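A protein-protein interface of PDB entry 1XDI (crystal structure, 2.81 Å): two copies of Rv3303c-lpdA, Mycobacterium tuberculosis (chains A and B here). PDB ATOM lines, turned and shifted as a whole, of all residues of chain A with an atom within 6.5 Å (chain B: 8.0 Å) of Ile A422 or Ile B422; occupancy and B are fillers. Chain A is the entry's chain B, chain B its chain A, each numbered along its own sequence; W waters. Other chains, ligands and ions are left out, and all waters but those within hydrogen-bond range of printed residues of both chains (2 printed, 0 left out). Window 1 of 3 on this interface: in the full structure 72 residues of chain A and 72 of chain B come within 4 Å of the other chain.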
ATOM      1  N   GLU A 361     -16.570 -21.299  31.038  1.00  0.00           N
ATOM      2  CA  GLU A 361     -16.995 -20.641  32.253  1.00  0.00           C
ATOM      3  C   GLU A 361     -18.448 -20.275  32.130  1.00  0.00           C
ATOM      4  O   GLU A 361     -18.955 -19.958  31.050  1.00  0.00           O
ATOM      5  CB  GLU A 361     -16.219 -19.361  32.457  1.00  0.00           C
ATOM      6  CG  GLU A 361     -14.711 -19.489  32.446  1.00  0.00           C
ATOM      7  CD  GLU A 361     -13.952 -18.235  32.970  1.00  0.00           C
ATOM      8  OE1 GLU A 361     -14.376 -17.056  32.759  1.00  0.00           O
ATOM      9  OE2 GLU A 361     -12.883 -18.446  33.586  1.00  0.00           O
ATOM     10  N   VAL A 418     -23.811 -15.923  30.500  1.00  0.00           N
ATOM     11  CA  VAL A 418     -22.817 -16.007  29.464  1.00  0.00           C
ATOM     12  C   VAL A 418     -22.087 -17.301  29.729  1.00  0.00           C
ATOM     13  O   VAL A 418     -21.738 -17.674  30.858  1.00  0.00           O
ATOM     14  CB  VAL A 418     -21.816 -14.841  29.514  1.00  0.00           C
ATOM     15  CG1 VAL A 418     -20.787 -14.966  28.378  1.00  0.00           C
ATOM     16  CG2 VAL A 418     -22.527 -13.566  29.360  1.00  0.00           C
ATOM     17  N   VAL A 419     -21.861 -17.981  28.634  1.00  0.00           N
ATOM     18  CA  VAL A 419     -21.183 -19.235  28.622  1.00  0.00           C
ATOM     19  C   VAL A 419     -20.186 -19.058  27.539  1.00  0.00           C
ATOM     20  O   VAL A 419     -20.521 -19.156  26.375  1.00  0.00           O
ATOM     21  CB  VAL A 419     -22.124 -20.369  28.202  1.00  0.00           C
ATOM     22  CG1 VAL A 419     -21.331 -21.666  28.079  1.00  0.00           C
ATOM     23  CG2 VAL A 419     -23.258 -20.502  29.216  1.00  0.00           C
ATOM     24  N   ALA A 420     -18.981 -18.718  27.915  1.00  0.00           N
ATOM     25  CA  ALA A 420     -17.921 -18.602  26.952  1.00  0.00           C
ATOM     26  C   ALA A 420     -16.593 -18.825  27.717  1.00  0.00           C
ATOM     27  O   ALA A 420     -16.604 -19.087  28.937  1.00  0.00           O
ATOM     28  CB  ALA A 420     -18.003 -17.269  26.282  1.00  0.00           C
ATOM     29  N   PRO A 421     -15.445 -18.795  27.017  1.00  0.00           N
ATOM     30  CA  PRO A 421     -14.152 -19.004  27.672  1.00  0.00           C
ATOM     31  C   PRO A 421     -13.771 -17.931  28.702  1.00  0.00           C
ATOM     32  O   PRO A 421     -12.990 -18.206  29.667  1.00  0.00           O
ATOM     33  CB  PRO A 421     -13.191 -19.061  26.515  1.00  0.00           C
ATOM     34  CG  PRO A 421     -14.006 -19.640  25.479  1.00  0.00           C
ATOM     35  CD  PRO A 421     -15.266 -18.875  25.567  1.00  0.00           C
ATOM     36  N   ILE A 422     -14.295 -16.720  28.526  1.00  0.00           N
ATOM     37  CA  ILE A 422     -13.985 -15.685  29.505  1.00  0.00           C
ATOM     38  C   ILE A 422     -15.285 -15.112  30.039  1.00  0.00           C
ATOM     39  O   ILE A 422     -15.390 -13.901  30.246  1.00  0.00           O
ATOM     40  CB  ILE A 422     -13.117 -14.521  28.892  1.00  0.00           C
ATOM     41  CG1 ILE A 422     -13.732 -14.035  27.582  1.00  0.00           C
ATOM     42  CG2 ILE A 422     -11.699 -14.968  28.692  1.00  0.00           C
ATOM     43  CD1 ILE A 422     -13.108 -12.767  27.089  1.00  0.00           C
ATOM     44  N   ALA A 423     -16.291 -15.961  30.242  1.00  0.00           N
ATOM     45  CA  ALA A 423     -17.559 -15.456  30.756  1.00  0.00           C
ATOM     46  C   ALA A 423     -17.270 -14.629  32.007  1.00  0.00           C
ATOM     47  O   ALA A 423     -17.908 -13.637  32.230  1.00  0.00           O
ATOM     48  CB  ALA A 423     -18.509 -16.587  31.061  1.00  0.00           C
ATOM     49  N   SER A 424     -16.259 -14.992  32.798  1.00  0.00           N
ATOM     50  CA  SER A 424     -15.980 -14.216  34.031  1.00  0.00           C
ATOM     51  C   SER A 424     -15.751 -12.722  33.786  1.00  0.00           C
ATOM     52  O   SER A 424     -16.049 -11.930  34.655  1.00  0.00           O
ATOM     53  CB  SER A 424     -14.817 -14.816  34.857  1.00  0.00           C
ATOM     54  OG  SER A 424     -13.549 -14.754  34.202  1.00  0.00           O
ATOM     55  N   GLU A 425     -15.239 -12.351  32.608  1.00  0.00           N
ATOM     56  CA  GLU A 425     -15.004 -10.931  32.219  1.00  0.00           C
ATOM     57  C   GLU A 425     -16.230 -10.400  31.419  1.00  0.00           C
ATOM     58  O   GLU A 425     -16.738  -9.316  31.719  1.00  0.00           O
ATOM     59  CB  GLU A 425     -13.757 -10.792  31.344  1.00  0.00           C
ATOM     60  CG  GLU A 425     -12.594 -11.631  31.781  1.00  0.00           C
ATOM     61  CD  GLU A 425     -11.915 -11.077  32.998  1.00  0.00           C
ATOM     62  OE1 GLU A 425     -12.317  -9.976  33.427  1.00  0.00           O
ATOM     63  OE2 GLU A 425     -10.977 -11.729  33.521  1.00  0.00           O
ATOM     64  N   LEU A 426     -16.726 -11.140  30.420  1.00  0.00           N
ATOM     65  CA  LEU A 426     -17.891 -10.668  29.669  1.00  0.00           C
ATOM     66  C   LEU A 426     -19.103 -10.320  30.521  1.00  0.00           C
ATOM     67  O   LEU A 426     -19.958  -9.553  30.098  1.00  0.00           O
ATOM     68  CB  LEU A 426     -18.338 -11.696  28.635  1.00  0.00           C
ATOM     69  CG  LEU A 426     -17.257 -11.955  27.590  1.00  0.00           C
ATOM     70  CD1 LEU A 426     -17.690 -13.111  26.640  1.00  0.00           C
ATOM     71  CD2 LEU A 426     -16.990 -10.666  26.859  1.00  0.00           C
ATOM     72  N   ILE A 427     -19.201 -10.857  31.723  1.00  0.00           N
ATOM     73  CA  ILE A 427     -20.364 -10.584  32.567  1.00  0.00           C
ATOM     74  C   ILE A 427     -20.393  -9.177  33.155  1.00  0.00           C
ATOM     75  O   ILE A 427     -21.519  -8.622  33.317  1.00  0.00           O
ATOM     76  CB  ILE A 427     -20.514 -11.642  33.712  1.00  0.00           C
ATOM     77  CG1 ILE A 427     -21.950 -11.629  34.231  1.00  0.00           C
ATOM     78  CG2 ILE A 427     -19.500 -11.432  34.812  1.00  0.00           C
ATOM     79  CD1 ILE A 427     -22.952 -12.256  33.273  1.00  0.00           C
ATOM     80  N   LEU A 453     -16.157 -10.790  21.419  1.00  0.00           N
ATOM     81  CA  LEU A 453     -17.227 -11.595  21.924  1.00  0.00           C
ATOM     82  C   LEU A 453     -18.281 -10.696  22.476  1.00  0.00           C
ATOM     83  O   LEU A 453     -19.482 -10.996  22.398  1.00  0.00           O
ATOM     84  CB  LEU A 453     -16.730 -12.521  23.020  1.00  0.00           C
ATOM     85  CG  LEU A 453     -16.052 -13.844  22.633  1.00  0.00           C
ATOM     86  CD1 LEU A 453     -15.809 -14.650  23.901  1.00  0.00           C
ATOM     87  CD2 LEU A 453     -16.894 -14.585  21.670  1.00  0.00           C
ATOM     88  N   THR B 355      -9.466  -0.973  19.554  1.00  0.00           N
ATOM     89  CA  THR B 355      -8.311  -1.697  20.042  1.00  0.00           C
ATOM     90  C   THR B 355      -7.347  -2.019  18.927  1.00  0.00           C
ATOM     91  O   THR B 355      -7.768  -2.149  17.791  1.00  0.00           O
ATOM     92  CB  THR B 355      -8.678  -3.027  20.695  1.00  0.00           C
ATOM     93  OG1 THR B 355      -8.326  -4.081  19.796  1.00  0.00           O
ATOM     94  CG2 THR B 355     -10.177  -3.127  21.026  1.00  0.00           C
ATOM     95  N   PHE B 357      -4.785  -4.817  17.748  1.00  0.00           N
ATOM     96  CA  PHE B 357      -4.574  -6.222  18.125  1.00  0.00           C
ATOM     97  C   PHE B 357      -3.122  -6.801  18.183  1.00  0.00           C
ATOM     98  O   PHE B 357      -2.779  -7.715  17.424  1.00  0.00           O
ATOM     99  CB  PHE B 357      -5.489  -7.112  17.285  1.00  0.00           C
ATOM    100  CG  PHE B 357      -6.928  -7.076  17.720  1.00  0.00           C
ATOM    101  CD1 PHE B 357      -7.371  -7.887  18.749  1.00  0.00           C
ATOM    102  CD2 PHE B 357      -7.851  -6.223  17.086  1.00  0.00           C
ATOM    103  CE1 PHE B 357      -8.712  -7.849  19.135  1.00  0.00           C
ATOM    104  CE2 PHE B 357      -9.192  -6.190  17.476  1.00  0.00           C
ATOM    105  CZ  PHE B 357      -9.614  -7.005  18.499  1.00  0.00           C
ATOM    106  N   THR B 358      -2.305  -6.275  19.112  1.00  0.00           N
ATOM    107  CA  THR B 358      -0.915  -6.708  19.331  1.00  0.00           C
ATOM    108  C   THR B 358      -0.922  -7.684  20.488  1.00  0.00           C
ATOM    109  O   THR B 358      -1.990  -8.134  20.914  1.00  0.00           O
ATOM    110  CB  THR B 358      -0.070  -5.529  19.773  1.00  0.00           C
ATOM    111  OG1 THR B 358      -0.951  -4.514  20.250  1.00  0.00           O
ATOM    112  CG2 THR B 358       0.736  -4.958  18.642  1.00  0.00           C
ATOM    113  N   PRO B 360       0.690  -7.478  24.120  1.00  0.00           N
ATOM    114  CA  PRO B 360      -0.731  -7.424  24.494  1.00  0.00           C
ATOM    115  C   PRO B 360      -1.596  -6.507  23.645  1.00  0.00           C
ATOM    116  O   PRO B 360      -1.099  -5.724  22.840  1.00  0.00           O
ATOM    117  CB  PRO B 360      -0.686  -6.905  25.916  1.00  0.00           C
ATOM    118  CG  PRO B 360       0.564  -6.014  25.899  1.00  0.00           C
ATOM    119  CD  PRO B 360       1.525  -6.908  25.197  1.00  0.00           C
ATOM    120  N   GLU B 361      -2.911  -6.607  23.868  1.00  0.00           N
ATOM    121  CA  GLU B 361      -3.902  -5.788  23.206  1.00  0.00           C
ATOM    122  C   GLU B 361      -3.928  -4.399  23.883  1.00  0.00           C
ATOM    123  O   GLU B 361      -3.546  -4.219  25.048  1.00  0.00           O
ATOM    124  CB  GLU B 361      -5.288  -6.450  23.329  1.00  0.00           C
ATOM    125  CG  GLU B 361      -5.574  -7.621  22.364  1.00  0.00           C
ATOM    126  CD  GLU B 361      -6.985  -8.259  22.526  1.00  0.00           C
ATOM    127  OE1 GLU B 361      -7.890  -7.605  23.105  1.00  0.00           O
ATOM    128  OE2 GLU B 361      -7.195  -9.407  22.051  1.00  0.00           O
ATOM    129  N   ILE B 362      -4.372  -3.408  23.131  1.00  0.00           N
ATOM    130  CA  ILE B 362      -4.528  -2.074  23.638  1.00  0.00           C
ATOM    131  C   ILE B 362      -5.881  -1.558  23.168  1.00  0.00           C
ATOM    132  O   ILE B 362      -6.166  -1.566  21.979  1.00  0.00           O
ATOM    133  CB  ILE B 362      -3.463  -1.185  23.088  1.00  0.00           C
ATOM    134  CG1 ILE B 362      -2.134  -1.914  23.198  1.00  0.00           C
ATOM    135  CG2 ILE B 362      -3.464   0.163  23.837  1.00  0.00           C
ATOM    136  CD1 ILE B 362      -0.952  -1.025  22.986  1.00  0.00           C
ATOM    137  N   ALA B 363      -6.727  -1.154  24.111  1.00  0.00           N
ATOM    138  CA  ALA B 363      -8.045  -0.582  23.800  1.00  0.00           C
ATOM    139  C   ALA B 363      -8.191   0.737  24.565  1.00  0.00           C
ATOM    140  O   ALA B 363      -7.670   0.894  25.676  1.00  0.00           O
ATOM    141  CB  ALA B 363      -9.183  -1.555  24.214  1.00  0.00           C
ATOM    142  N   LEU B 386      -1.831  -3.880  36.236  1.00  0.00           N
ATOM    143  CA  LEU B 386      -2.638  -5.093  36.386  1.00  0.00           C
ATOM    144  C   LEU B 386      -1.870  -6.188  37.129  1.00  0.00           C
ATOM    145  O   LEU B 386      -2.468  -7.179  37.585  1.00  0.00           O
ATOM    146  CB  LEU B 386      -3.083  -5.650  35.014  1.00  0.00           C
ATOM    147  CG  LEU B 386      -4.344  -5.007  34.435  1.00  0.00           C
ATOM    148  CD1 LEU B 386      -4.571  -5.270  32.944  1.00  0.00           C
ATOM    149  CD2 LEU B 386      -5.462  -5.519  35.283  1.00  0.00           C
ATOM    150  N   ARG B 391      -5.722 -12.527  38.789  1.00  0.00           N
ATOM    151  CA  ARG B 391      -6.000 -13.073  37.464  1.00  0.00           C
ATOM    152  C   ARG B 391      -4.796 -12.784  36.583  1.00  0.00           C
ATOM    153  O   ARG B 391      -4.250 -13.705  35.967  1.00  0.00           O
ATOM    154  CB  ARG B 391      -7.284 -12.440  36.883  1.00  0.00           C
ATOM    155  CG  ARG B 391      -7.598 -12.759  35.400  1.00  0.00           C
ATOM    156  CD  ARG B 391      -7.581 -14.263  35.091  1.00  0.00           C
ATOM    157  NE  ARG B 391      -8.644 -14.976  35.776  1.00  0.00           N
ATOM    158  CZ  ARG B 391      -8.626 -16.281  35.975  1.00  0.00           C
ATOM    159  NH1 ARG B 391      -7.585 -16.988  35.550  1.00  0.00           N
ATOM    160  NH2 ARG B 391      -9.649 -16.875  36.547  1.00  0.00           N
ATOM    161  N   SER B 395      -2.361 -15.244  34.266  1.00  0.00           N
ATOM    162  CA  SER B 395      -2.052 -15.170  32.808  1.00  0.00           C
ATOM    163  C   SER B 395      -0.646 -14.554  32.548  1.00  0.00           C
ATOM    164  O   SER B 395      -0.332 -14.040  31.456  1.00  0.00           O
ATOM    165  CB  SER B 395      -3.096 -14.341  32.063  1.00  0.00           C
ATOM    166  OG  SER B 395      -4.409 -14.564  32.562  1.00  0.00           O
ATOM    167  N   MET B 397       0.954 -11.800  33.232  1.00  0.00           N
ATOM    168  CA  MET B 397       0.969 -10.445  32.688  1.00  0.00           C
ATOM    169  C   MET B 397       1.759  -9.620  33.658  1.00  0.00           C
ATOM    170  O   MET B 397       1.454  -9.602  34.856  1.00  0.00           O
ATOM    171  CB  MET B 397      -0.419  -9.829  32.649  1.00  0.00           C
ATOM    172  CG  MET B 397      -1.448 -10.567  31.852  1.00  0.00           C
ATOM    173  SD  MET B 397      -3.044  -9.788  32.065  1.00  0.00           S
ATOM    174  CE  MET B 397      -4.063 -11.201  32.012  1.00  0.00           C
ATOM    175  N   VAL B 418      -7.129   0.455  28.275  1.00  0.00           N
ATOM    176  CA  VAL B 418      -6.859  -0.864  28.834  1.00  0.00           C
ATOM    177  C   VAL B 418      -5.845  -1.544  27.967  1.00  0.00           C
ATOM    178  O   VAL B 418      -6.063  -1.685  26.754  1.00  0.00           O
ATOM    179  CB  VAL B 418      -8.108  -1.796  28.841  1.00  0.00           C
ATOM    180  CG1 VAL B 418      -7.767  -3.078  29.501  1.00  0.00           C
ATOM    181  CG2 VAL B 418      -9.233  -1.179  29.564  1.00  0.00           C
ATOM    182  N   VAL B 419      -4.740  -1.930  28.587  1.00  0.00           N
ATOM    183  CA  VAL B 419      -3.721  -2.669  27.908  1.00  0.00           C
ATOM    184  C   VAL B 419      -3.631  -4.036  28.595  1.00  0.00           C
ATOM    185  O   VAL B 419      -3.123  -4.118  29.715  1.00  0.00           O
ATOM    186  CB  VAL B 419      -2.385  -1.939  27.998  1.00  0.00           C
ATOM    187  CG1 VAL B 419      -1.221  -2.875  27.697  1.00  0.00           C
ATOM    188  CG2 VAL B 419      -2.379  -0.830  27.005  1.00  0.00           C
ATOM    189  N   ALA B 420      -4.149  -5.089  27.957  1.00  0.00           N
ATOM    190  CA  ALA B 420      -4.075  -6.467  28.494  1.00  0.00           C
ATOM    191  C   ALA B 420      -4.373  -7.487  27.384  1.00  0.00           C
ATOM    192  O   ALA B 420      -4.751  -7.096  26.254  1.00  0.00           O
ATOM    193  CB  ALA B 420      -5.032  -6.654  29.615  1.00  0.00           C
ATOM    194  N   PRO B 421      -4.236  -8.804  27.676  1.00  0.00           N
ATOM    195  CA  PRO B 421      -4.496  -9.782  26.611  1.00  0.00           C
ATOM    196  C   PRO B 421      -5.879  -9.721  25.980  1.00  0.00           C
ATOM    197  O   PRO B 421      -6.004  -9.963  24.766  1.00  0.00           O
ATOM    198  CB  PRO B 421      -4.209 -11.121  27.272  1.00  0.00           C
ATOM    199  CG  PRO B 421      -3.309 -10.762  28.438  1.00  0.00           C
ATOM    200  CD  PRO B 421      -3.877  -9.487  28.930  1.00  0.00           C
ATOM    201  N   ILE B 422      -6.917  -9.388  26.764  1.00  0.00           N
ATOM    202  CA  ILE B 422      -8.257  -9.292  26.182  1.00  0.00           C
ATOM    203  C   ILE B 422      -8.810  -7.886  26.322  1.00  0.00           C
ATOM    204  O   ILE B 422      -9.939  -7.692  26.722  1.00  0.00           O
ATOM    205  CB  ILE B 422      -9.246 -10.294  26.865  1.00  0.00           C
ATOM    206  CG1 ILE B 422      -9.166 -10.148  28.370  1.00  0.00           C
ATOM    207  CG2 ILE B 422      -8.983 -11.731  26.397  1.00  0.00           C
ATOM    208  CD1 ILE B 422     -10.118 -11.064  29.060  1.00  0.00           C
ATOM    209  N   ALA B 423      -8.018  -6.886  26.003  1.00  0.00           N
ATOM    210  CA  ALA B 423      -8.505  -5.537  26.201  1.00  0.00           C
ATOM    211  C   ALA B 423      -9.736  -5.270  25.340  1.00  0.00           C
ATOM    212  O   ALA B 423     -10.666  -4.557  25.767  1.00  0.00           O
ATOM    213  CB  ALA B 423      -7.409  -4.520  25.890  1.00  0.00           C
ATOM    214  N   SER B 424      -9.740  -5.864  24.143  1.00  0.00           N
ATOM    215  CA  SER B 424     -10.825  -5.669  23.201  1.00  0.00           C
ATOM    216  C   SER B 424     -12.192  -6.034  23.815  1.00  0.00           C
ATOM    217  O   SER B 424     -13.204  -5.532  23.368  1.00  0.00           O
ATOM    218  CB  SER B 424     -10.553  -6.462  21.916  1.00  0.00           C
ATOM    219  OG  SER B 424     -10.500  -7.862  22.167  1.00  0.00           O
ATOM    220  N   GLU B 425     -12.203  -6.880  24.837  1.00  0.00           N
ATOM    221  CA  GLU B 425     -13.427  -7.268  25.536  1.00  0.00           C
ATOM    222  C   GLU B 425     -13.668  -6.372  26.764  1.00  0.00           C
ATOM    223  O   GLU B 425     -14.757  -5.837  26.926  1.00  0.00           O
ATOM    224  CB  GLU B 425     -13.363  -8.720  26.024  1.00  0.00           C
ATOM    225  CG  GLU B 425     -12.933  -9.767  24.986  1.00  0.00           C
ATOM    226  CD  GLU B 425     -13.951  -9.993  23.880  1.00  0.00           C
ATOM    227  OE1 GLU B 425     -14.973  -9.287  23.920  1.00  0.00           O
ATOM    228  OE2 GLU B 425     -13.720 -10.860  22.995  1.00  0.00           O
ATOM    229  N   LEU B 426     -12.654  -6.221  27.623  1.00  0.00           N
ATOM    230  CA  LEU B 426     -12.757  -5.401  28.836  1.00  0.00           C
ATOM    231  C   LEU B 426     -13.019  -3.917  28.576  1.00  0.00           C
ATOM    232  O   LEU B 426     -13.408  -3.193  29.501  1.00  0.00           O
ATOM    233  CB  LEU B 426     -11.479  -5.434  29.640  1.00  0.00           C
ATOM    234  CG  LEU B 426     -10.746  -6.727  29.800  1.00  0.00           C
ATOM    235  CD1 LEU B 426      -9.316  -6.454  30.153  1.00  0.00           C
ATOM    236  CD2 LEU B 426     -11.426  -7.506  30.875  1.00  0.00           C
ATOM    237  N   ILE B 427     -12.774  -3.422  27.366  1.00  0.00           N
ATOM    238  CA  ILE B 427     -12.997  -2.005  27.131  1.00  0.00           C
ATOM    239  C   ILE B 427     -14.487  -1.714  27.188  1.00  0.00           C
ATOM    240  O   ILE B 427     -14.890  -0.625  27.631  1.00  0.00           O
ATOM    241  CB  ILE B 427     -12.417  -1.554  25.748  1.00  0.00           C
ATOM    242  CG1 ILE B 427     -12.314  -0.032  25.665  1.00  0.00           C
ATOM    243  CG2 ILE B 427     -13.291  -2.010  24.652  1.00  0.00           C
ATOM    244  CD1 ILE B 427     -11.332   0.571  26.628  1.00  0.00           C
ATOM    245  N   LEU B 428     -15.302  -2.706  26.797  1.00  0.00           N
ATOM    246  CA  LEU B 428     -16.762  -2.539  26.735  1.00  0.00           C
ATOM    247  C   LEU B 428     -17.395  -1.861  27.938  1.00  0.00           C
ATOM    248  O   LEU B 428     -18.047  -0.825  27.795  1.00  0.00           O
ATOM    249  CB  LEU B 428     -17.485  -3.869  26.448  1.00  0.00           C
ATOM    250  CG  LEU B 428     -19.004  -3.645  26.270  1.00  0.00           C
ATOM    251  CD1 LEU B 428     -19.237  -2.539  25.258  1.00  0.00           C
ATOM    252  CD2 LEU B 428     -19.692  -4.902  25.849  1.00  0.00           C
ATOM    253  N   SER B 452     -10.792 -11.670  38.428  1.00  0.00           N
ATOM    254  CA  SER B 452     -10.844 -11.376  37.010  1.00  0.00           C
ATOM    255  C   SER B 452     -10.116 -10.050  36.813  1.00  0.00           C
ATOM    256  O   SER B 452      -9.900  -9.325  37.789  1.00  0.00           O
ATOM    257  CB  SER B 452     -12.309 -11.250  36.537  1.00  0.00           C
ATOM    258  OG  SER B 452     -12.960 -10.163  37.171  1.00  0.00           O
ATOM    259  N   LEU B 453      -9.734  -9.726  35.579  1.00  0.00           N
ATOM    260  CA  LEU B 453      -9.070  -8.455  35.381  1.00  0.00           C
ATOM    261  C   LEU B 453     -10.161  -7.374  35.418  1.00  0.00           C
ATOM    262  O   LEU B 453      -9.893  -6.221  35.744  1.00  0.00           O
ATOM    263  CB  LEU B 453      -8.332  -8.446  34.044  1.00  0.00           C
ATOM    264  CG  LEU B 453      -7.471  -9.690  33.778  1.00  0.00           C
ATOM    265  CD1 LEU B 453      -7.017  -9.724  32.317  1.00  0.00           C
ATOM    266  CD2 LEU B 453      -6.318  -9.693  34.688  1.00  0.00           C
ATOM    267  N   SER B 454     -11.407  -7.721  35.130  1.00  0.00           N
ATOM    268  CA  SER B 454     -12.403  -6.677  35.183  1.00  0.00           C
ATOM    269  C   SER B 454     -12.642  -6.171  36.612  1.00  0.00           C
ATOM    270  O   SER B 454     -13.288  -5.151  36.805  1.00  0.00           O
ATOM    271  CB  SER B 454     -13.715  -7.155  34.603  1.00  0.00           C
ATOM    272  OG  SER B 454     -14.470  -7.792  35.610  1.00  0.00           O
HETATM  273  O   HOH W   1     -10.980 -13.936  34.942  1.00  0.00           O
HETATM  274  O   HOH W   2      -8.898 -13.753  32.593  1.00  0.00           O
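The backbone NH (N) of Leu A453 lies within hydrogen-bond range of the side-chain carboxylate (OE2) of Glu B425 (2.9 Å). OE1 of Glu A425 lies within hydrogen-bond range of N of Ser B454, 3.0 Å away. The backbone NH (N) of Leu B453 is in hydrogen-bond range of the side-chain carboxylate (OE2) of Glu A425 (3.1 Å).
The side-chain hydroxyl (OG) of Ser B454 is in hydrogen-bond range of the side-chain hydroxyl (OG) of Ser B452.
Ile A422 touches just these residues of chain B: Ile B422 (3.97 Å) and Glu B425 (3.7 Å). Of the printed residues of chain A, Ile B422 touches Ile A422 and Glu A425. No residue of chain B comes within 4 Å of Ala A423. Printed residues of chain B within 4 Å of Leu A453: Glu B425 (2.9 Å). Of the printed residues of chain B, Leu A426 touches Glu B425. Of the printed residues of chain A, Leu B453 touches Glu A425. Ser A424 touches none of the printed residues of chain B. Ala A420 touches none of the printed residues of chain B. The nearest residue of chain B that does not touch Ile A422 is Leu B426 (6.6 Å). The nearest printed residue of chain A that does not touch Ile B422 is Leu A426 (6.7 Å).
Among the printed residues, pairs that only touch across the chains: Ile A422 with Ile B422 (3.97 Å), Ile A422 with Glu B425 (3.7 Å), Glu A425 with Ile B422 (3.7 Å), Glu A425 with Leu B426 (3.7 Å), Glu A425 with Ser B452 (3.3 Å) and Leu A426 with Glu B425 (3.8 Å).
Ile B422 touches its own counterpart, Ile A422. Ile A422 touches Glu B425, and with the chains exchanged Glu A425 touches Ile B422. Glu A425 touches Leu B426, and with the chains exchanged Leu A426 touches Glu B425. Glu A425 touches Leu B453, and with the chains exchanged Leu A453 touches Glu B425. Positions printed for both chains: 361, 418, 419, 420, 421, 422, 423, 424, 425, 426, 427 and 453. Of the 9 pairs that touch across the chains among the printed residues, 7 have their exchanged pair printed and touching as well.
Water W1 lies within hydrogen-bond range of OE2 of Glu A425, NE of Arg B391 and OG of Ser A424. Water W2 bridges the side-chain carboxylate of Glu A425 and the guanidinium group of Arg B391.
Printed residues of chain B that touch a printed residue of chain A: Ile B422, Glu B425, Leu B426, Ser B452, Leu B453 and Ser B454. Hydrophobic or aromatic side chains of chain B within 4 Å of the printed part of chain A: Ile B422 and Leu B426. Of the 12 printed residues of chain A, 4 touch a printed residue of chain B. Printed residues of chain A that touch a printed residue of chain B: Ile A422, Glu A425, Leu A426 and Leu A453. Hydrophobic or aromatic side chains of chain A within 4 Å of the printed part of chain B: Ile A422, Leu A426 and Leu A453.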
